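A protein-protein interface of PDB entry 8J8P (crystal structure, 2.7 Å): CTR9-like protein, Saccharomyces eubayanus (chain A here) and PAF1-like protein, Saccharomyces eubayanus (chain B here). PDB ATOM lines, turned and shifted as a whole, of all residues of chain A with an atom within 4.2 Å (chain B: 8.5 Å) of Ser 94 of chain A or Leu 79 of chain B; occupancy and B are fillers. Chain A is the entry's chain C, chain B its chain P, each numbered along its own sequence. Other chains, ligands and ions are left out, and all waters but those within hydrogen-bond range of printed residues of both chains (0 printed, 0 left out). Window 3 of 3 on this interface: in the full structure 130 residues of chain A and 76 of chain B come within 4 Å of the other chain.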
ATOM      1  N   LYS A  57      -6.433  25.548  20.100  1.00  0.00           N
ATOM      2  CA  LYS A  57      -5.182  25.968  19.470  1.00  0.00           C
ATOM      3  C   LYS A  57      -3.989  25.156  19.968  1.00  0.00           C
ATOM      4  O   LYS A  57      -3.067  24.837  19.196  1.00  0.00           O
ATOM      5  CB  LYS A  57      -4.971  27.456  19.736  1.00  0.00           C
ATOM      6  CG  LYS A  57      -3.872  28.103  18.930  1.00  0.00           C
ATOM      7  CD  LYS A  57      -3.904  29.603  19.165  1.00  0.00           C
ATOM      8  CE  LYS A  57      -3.869  29.897  20.652  1.00  0.00           C
ATOM      9  NZ  LYS A  57      -3.713  31.349  20.936  1.00  0.00           N
ATOM     10  N   LEU A  61      -0.486  23.688  18.157  1.00  0.00           N
ATOM     11  CA  LEU A  61       0.881  23.985  18.578  1.00  0.00           C
ATOM     12  C   LEU A  61       1.626  22.725  19.010  1.00  0.00           C
ATOM     13  O   LEU A  61       2.820  22.580  18.730  1.00  0.00           O
ATOM     14  CB  LEU A  61       0.867  25.013  19.704  1.00  0.00           C
ATOM     15  CG  LEU A  61       0.486  26.424  19.275  1.00  0.00           C
ATOM     16  CD1 LEU A  61       0.099  27.247  20.489  1.00  0.00           C
ATOM     17  CD2 LEU A  61       1.638  27.064  18.529  1.00  0.00           C
ATOM     18  N   ARG A  92      -4.110  34.858  17.797  1.00  0.00           N
ATOM     19  CA  ARG A  92      -2.950  34.758  16.919  1.00  0.00           C
ATOM     20  C   ARG A  92      -1.633  34.845  17.683  1.00  0.00           C
ATOM     21  O   ARG A  92      -0.611  34.368  17.178  1.00  0.00           O
ATOM     22  CB  ARG A  92      -2.978  35.867  15.860  1.00  0.00           C
ATOM     23  CG  ARG A  92      -4.211  35.911  14.972  1.00  0.00           C
ATOM     24  CD  ARG A  92      -3.912  36.602  13.646  1.00  0.00           C
ATOM     25  NE  ARG A  92      -4.367  35.817  12.501  1.00  0.00           N
ATOM     26  CZ  ARG A  92      -3.924  35.984  11.259  1.00  0.00           C
ATOM     27  NH1 ARG A  92      -3.006  36.907  10.999  1.00  0.00           N
ATOM     28  NH2 ARG A  92      -4.396  35.226  10.276  1.00  0.00           N
ATOM     29  N   ALA A  93      -1.643  35.437  18.883  1.00  0.00           N
ATOM     30  CA  ALA A  93      -0.407  35.802  19.573  1.00  0.00           C
ATOM     31  C   ALA A  93       0.532  34.613  19.729  1.00  0.00           C
ATOM     32  O   ALA A  93       1.699  34.666  19.317  1.00  0.00           O
ATOM     33  CB  ALA A  93      -0.741  36.403  20.940  1.00  0.00           C
ATOM     34  N   SER A  94       0.035  33.527  20.325  1.00  0.00           N
ATOM     35  CA  SER A  94       0.864  32.347  20.541  1.00  0.00           C
ATOM     36  C   SER A  94       1.376  31.766  19.230  1.00  0.00           C
ATOM     37  O   SER A  94       2.485  31.219  19.184  1.00  0.00           O
ATOM     38  CB  SER A  94       0.071  31.293  21.309  1.00  0.00           C
ATOM     39  OG  SER A  94      -0.152  31.726  22.635  1.00  0.00           O
ATOM     40  N   LEU A  95       0.585  31.867  18.160  1.00  0.00           N
ATOM     41  CA  LEU A  95       1.040  31.384  16.860  1.00  0.00           C
ATOM     42  C   LEU A  95       2.223  32.202  16.357  1.00  0.00           C
ATOM     43  O   LEU A  95       3.197  31.647  15.831  1.00  0.00           O
ATOM     44  CB  LEU A  95      -0.112  31.425  15.858  1.00  0.00           C
ATOM     45  CG  LEU A  95      -1.442  30.920  16.411  1.00  0.00           C
ATOM     46  CD1 LEU A  95      -2.590  31.393  15.539  1.00  0.00           C
ATOM     47  CD2 LEU A  95      -1.422  29.399  16.506  1.00  0.00           C
ATOM     48  N   HIS A  96       2.163  33.523  16.524  1.00  0.00           N
ATOM     49  CA  HIS A  96       3.300  34.348  16.143  1.00  0.00           C
ATOM     50  C   HIS A  96       4.514  34.053  17.018  1.00  0.00           C
ATOM     51  O   HIS A  96       5.651  34.074  16.535  1.00  0.00           O
ATOM     52  CB  HIS A  96       2.912  35.823  16.205  1.00  0.00           C
ATOM     53  CG  HIS A  96       2.092  36.268  15.034  1.00  0.00           C
ATOM     54  ND1 HIS A  96       2.556  36.202  13.738  1.00  0.00           N
ATOM     55  CD2 HIS A  96       0.835  36.766  14.960  1.00  0.00           C
ATOM     56  CE1 HIS A  96       1.623  36.649  12.916  1.00  0.00           C
ATOM     57  NE2 HIS A  96       0.570  36.997  13.631  1.00  0.00           N
ATOM     58  N   THR A  97       4.295  33.748  18.300  1.00  0.00           N
ATOM     59  CA  THR A  97       5.403  33.363  19.173  1.00  0.00           C
ATOM     60  C   THR A  97       6.078  32.086  18.675  1.00  0.00           C
ATOM     61  O   THR A  97       7.317  32.012  18.565  1.00  0.00           O
ATOM     62  CB  THR A  97       4.891  33.187  20.605  1.00  0.00           C
ATOM     63  OG1 THR A  97       4.443  34.451  21.113  1.00  0.00           O
ATOM     64  CG2 THR A  97       5.985  32.646  21.503  1.00  0.00           C
ATOM     65  N   PHE A  98       5.270  31.064  18.373  1.00  0.00           N
ATOM     66  CA  PHE A  98       5.825  29.829  17.833  1.00  0.00           C
ATOM     67  C   PHE A  98       6.585  30.090  16.545  1.00  0.00           C
ATOM     68  O   PHE A  98       7.659  29.519  16.324  1.00  0.00           O
ATOM     69  CB  PHE A  98       4.729  28.797  17.575  1.00  0.00           C
ATOM     70  CG  PHE A  98       5.226  27.575  16.847  1.00  0.00           C
ATOM     71  CD1 PHE A  98       5.232  27.524  15.458  1.00  0.00           C
ATOM     72  CD2 PHE A  98       5.702  26.483  17.553  1.00  0.00           C
ATOM     73  CE1 PHE A  98       5.705  26.406  14.791  1.00  0.00           C
ATOM     74  CE2 PHE A  98       6.170  25.355  16.894  1.00  0.00           C
ATOM     75  CZ  PHE A  98       6.173  25.315  15.512  1.00  0.00           C
ATOM     76  N   TRP A 138       4.337  38.577  27.508  1.00  0.00           N
ATOM     77  CA  TRP A 138       4.596  37.143  27.590  1.00  0.00           C
ATOM     78  C   TRP A 138       6.097  36.865  27.601  1.00  0.00           C
ATOM     79  O   TRP A 138       6.876  37.535  26.916  1.00  0.00           O
ATOM     80  CB  TRP A 138       3.933  36.432  26.407  1.00  0.00           C
ATOM     81  CG  TRP A 138       4.198  34.962  26.326  1.00  0.00           C
ATOM     82  CD1 TRP A 138       4.587  34.257  25.219  1.00  0.00           C
ATOM     83  CD2 TRP A 138       4.070  34.007  27.388  1.00  0.00           C
ATOM     84  NE1 TRP A 138       4.718  32.920  25.531  1.00  0.00           N
ATOM     85  CE2 TRP A 138       4.406  32.744  26.856  1.00  0.00           C
ATOM     86  CE3 TRP A 138       3.707  34.099  28.739  1.00  0.00           C
ATOM     87  CZ2 TRP A 138       4.397  31.581  27.631  1.00  0.00           C
ATOM     88  CZ3 TRP A 138       3.694  32.945  29.506  1.00  0.00           C
ATOM     89  CH2 TRP A 138       4.039  31.701  28.948  1.00  0.00           C
ATOM     90  N   PHE B  72      11.145  22.991  26.133  1.00  0.00           N
ATOM     91  CA  PHE B  72      10.447  23.172  27.406  1.00  0.00           C
ATOM     92  C   PHE B  72       8.971  22.842  27.217  1.00  0.00           C
ATOM     93  O   PHE B  72       8.183  23.700  26.789  1.00  0.00           O
ATOM     94  CB  PHE B  72      10.644  24.598  27.918  1.00  0.00           C
ATOM     95  CG  PHE B  72      12.096  25.001  28.009  1.00  0.00           C
ATOM     96  CD1 PHE B  72      12.782  24.893  29.204  1.00  0.00           C
ATOM     97  CD2 PHE B  72      12.777  25.459  26.892  1.00  0.00           C
ATOM     98  CE1 PHE B  72      14.116  25.244  29.285  1.00  0.00           C
ATOM     99  CE2 PHE B  72      14.110  25.813  26.969  1.00  0.00           C
ATOM    100  CZ  PHE B  72      14.780  25.698  28.165  1.00  0.00           C
ATOM    101  N   PRO B  73       8.558  21.605  27.512  1.00  0.00           N
ATOM    102  CA  PRO B  73       7.145  21.232  27.347  1.00  0.00           C
ATOM    103  C   PRO B  73       6.208  22.176  28.090  1.00  0.00           C
ATOM    104  O   PRO B  73       6.504  22.635  29.195  1.00  0.00           O
ATOM    105  CB  PRO B  73       7.089  19.815  27.929  1.00  0.00           C
ATOM    106  CG  PRO B  73       8.471  19.275  27.744  1.00  0.00           C
ATOM    107  CD  PRO B  73       9.404  20.454  27.883  1.00  0.00           C
ATOM    108  N   GLY B  74       5.066  22.467  27.464  1.00  0.00           N
ATOM    109  CA  GLY B  74       4.086  23.364  28.025  1.00  0.00           C
ATOM    110  C   GLY B  74       4.279  24.827  27.680  1.00  0.00           C
ATOM    111  O   GLY B  74       3.331  25.609  27.815  1.00  0.00           O
ATOM    112  N   LEU B  75       5.467  25.219  27.218  1.00  0.00           N
ATOM    113  CA  LEU B  75       5.776  26.641  27.085  1.00  0.00           C
ATOM    114  C   LEU B  75       5.145  27.251  25.836  1.00  0.00           C
ATOM    115  O   LEU B  75       4.366  28.206  25.926  1.00  0.00           O
ATOM    116  CB  LEU B  75       7.290  26.850  27.069  1.00  0.00           C
ATOM    117  CG  LEU B  75       7.726  28.315  27.087  1.00  0.00           C
ATOM    118  CD1 LEU B  75       6.978  29.082  28.151  1.00  0.00           C
ATOM    119  CD2 LEU B  75       9.218  28.408  27.328  1.00  0.00           C
ATOM    120  N   LEU B  76       5.487  26.731  24.661  1.00  0.00           N
ATOM    121  CA  LEU B  76       5.000  27.300  23.410  1.00  0.00           C
ATOM    122  C   LEU B  76       3.627  26.782  22.996  1.00  0.00           C
ATOM    123  O   LEU B  76       2.995  27.390  22.125  1.00  0.00           O
ATOM    124  CB  LEU B  76       5.995  27.032  22.275  1.00  0.00           C
ATOM    125  CG  LEU B  76       7.364  27.702  22.412  1.00  0.00           C
ATOM    126  CD1 LEU B  76       8.323  27.173  21.359  1.00  0.00           C
ATOM    127  CD2 LEU B  76       7.254  29.219  22.339  1.00  0.00           C
ATOM    128  N   ASN B  77       3.154  25.679  23.579  1.00  0.00           N
ATOM    129  CA  ASN B  77       1.850  25.132  23.223  1.00  0.00           C
ATOM    130  C   ASN B  77       0.770  25.460  24.250  1.00  0.00           C
ATOM    131  O   ASN B  77      -0.314  25.921  23.877  1.00  0.00           O
ATOM    132  CB  ASN B  77       1.950  23.613  23.011  1.00  0.00           C
ATOM    133  CG  ASN B  77       2.467  22.875  24.235  1.00  0.00           C
ATOM    134  OD1 ASN B  77       3.120  23.460  25.098  1.00  0.00           O
ATOM    135  ND2 ASN B  77       2.185  21.574  24.308  1.00  0.00           N
ATOM    136  N   LYS B  78       1.042  25.249  25.537  1.00  0.00           N
ATOM    137  CA  LYS B  78       0.056  25.498  26.579  1.00  0.00           C
ATOM    138  C   LYS B  78       0.324  26.764  27.383  1.00  0.00           C
ATOM    139  O   LYS B  78      -0.414  27.040  28.335  1.00  0.00           O
ATOM    140  CB  LYS B  78      -0.023  24.300  27.533  1.00  0.00           C
ATOM    141  CG  LYS B  78      -0.347  22.982  26.850  1.00  0.00           C
ATOM    142  CD  LYS B  78      -0.334  21.830  27.849  1.00  0.00           C
ATOM    143  CE  LYS B  78      -0.621  20.495  27.169  1.00  0.00           C
ATOM    144  NZ  LYS B  78      -0.298  19.333  28.051  1.00  0.00           N
ATOM    145  N   LEU B  79       1.358  27.532  27.041  1.00  0.00           N
ATOM    146  CA  LEU B  79       1.689  28.765  27.764  1.00  0.00           C
ATOM    147  C   LEU B  79       1.969  28.507  29.247  1.00  0.00           C
ATOM    148  O   LEU B  79       1.670  29.340  30.106  1.00  0.00           O
ATOM    149  CB  LEU B  79       0.585  29.810  27.599  1.00  0.00           C
ATOM    150  CG  LEU B  79       0.891  30.853  26.525  1.00  0.00           C
ATOM    151  CD1 LEU B  79       0.787  30.220  25.147  1.00  0.00           C
ATOM    152  CD2 LEU B  79      -0.036  32.049  26.657  1.00  0.00           C
ATOM    153  N   ASP B  80       2.553  27.347  29.554  1.00  0.00           N
ATOM    154  CA  ASP B  80       2.964  26.999  30.915  1.00  0.00           C
ATOM    155  C   ASP B  80       4.477  27.173  31.005  1.00  0.00           C
ATOM    156  O   ASP B  80       5.240  26.296  30.590  1.00  0.00           O
ATOM    157  CB  ASP B  80       2.547  25.574  31.271  1.00  0.00           C
ATOM    158  CG  ASP B  80       2.988  25.167  32.673  1.00  0.00           C
ATOM    159  OD1 ASP B  80       3.274  26.064  33.500  1.00  0.00           O
ATOM    160  OD2 ASP B  80       3.056  23.947  32.945  1.00  0.00           O
ATOM    161  N   SER B  81       4.910  28.304  31.565  1.00  0.00           N
ATOM    162  CA  SER B  81       6.321  28.647  31.654  1.00  0.00           C
ATOM    163  C   SER B  81       7.005  28.025  32.862  1.00  0.00           C
ATOM    164  O   SER B  81       8.087  28.484  33.253  1.00  0.00           O
ATOM    165  CB  SER B  81       6.487  30.164  31.699  1.00  0.00           C
ATOM    166  OG  SER B  81       6.058  30.661  32.954  1.00  0.00           O
ATOM    167  N   LYS B  82       6.402  27.002  33.462  1.00  0.00           N
ATOM    168  CA  LYS B  82       6.936  26.451  34.703  1.00  0.00           C
ATOM    169  C   LYS B  82       8.359  25.934  34.511  1.00  0.00           C
ATOM    170  O   LYS B  82       9.266  26.264  35.289  1.00  0.00           O
ATOM    171  CB  LYS B  82       5.999  25.353  35.211  1.00  0.00           C
ATOM    172  CG  LYS B  82       6.659  24.259  36.029  1.00  0.00           C
ATOM    173  CD  LYS B  82       5.667  23.128  36.309  1.00  0.00           C
ATOM    174  CE  LYS B  82       5.082  22.564  35.013  1.00  0.00           C
ATOM    175  NZ  LYS B  82       3.789  21.844  35.230  1.00  0.00           N
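Leu 61 of chain A touches Leu 76 of chain B.
Asn 77 of chain B touches Leu 61 of chain A.
Leu 79 of chain B touches Ser 94 of chain A.
Thr 97 of chain A touches Leu 76 of chain B.
Trp 138 of chain A touches Leu 75 of chain B.
Leu 79 of chain B touches Trp 138 of chain A.
Ser 81 of chain B touches Trp 138 of chain A.
The backbone carbonyl oxygen (O) of Ala 93 of chain A lies within hydrogen-bond range of the side-chain hydroxyl (OG1) of Thr 97 of chain A (3.3 Å).
OD1 of Asn 77 of chain B sits close to N of Gly 74 of chain B (3.2 Å).
The backbone carbonyl oxygen (O) of Gly 74 of chain B lies within hydrogen-bond range of the backbone NH (N) of Leu 79 of chain B (2.9 Å).
Hydrophobic or aromatic side chains of chain B within 4 Å of the printed part of chain A: Leu 75, Leu 76 and Leu 79.
Of the 10 printed residues of chain A, 4 touch a printed residue of chain B.
Printed residues of chain A that touch a printed residue of chain B: Leu 61, Ser 94, Thr 97 and Trp 138.
Hydrophobic or aromatic side chains of chain A within 4 Å of the printed part of chain B: Leu 61 and Trp 138.
Among the printed residues, 7 pairs touch across the chains.
No residue of chain B comes within 4 Å of Ala 93 of chain A.
Of the printed residues of chain A, Leu 75 of chain B touches Trp 138.
Of the printed residues of chain A, Leu 76 of chain B touches Leu 61 (3.3 Å) and Thr 97 (3.7 Å).
Of chain A, only Ser 94 and Trp 138 come within 4 Å of Leu 79 of chain B.
Of the printed residues of chain A, Ser 81 of chain B touches Trp 138 (3.99 Å).
The nearest printed residue of chain A that does not touch Leu 79 of chain B is Leu 61 of chain A (5.6 Å).
The nearest printed residue of chain B that does not touch Leu 61 of chain A is Lys 78 of chain B (5.5 Å).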
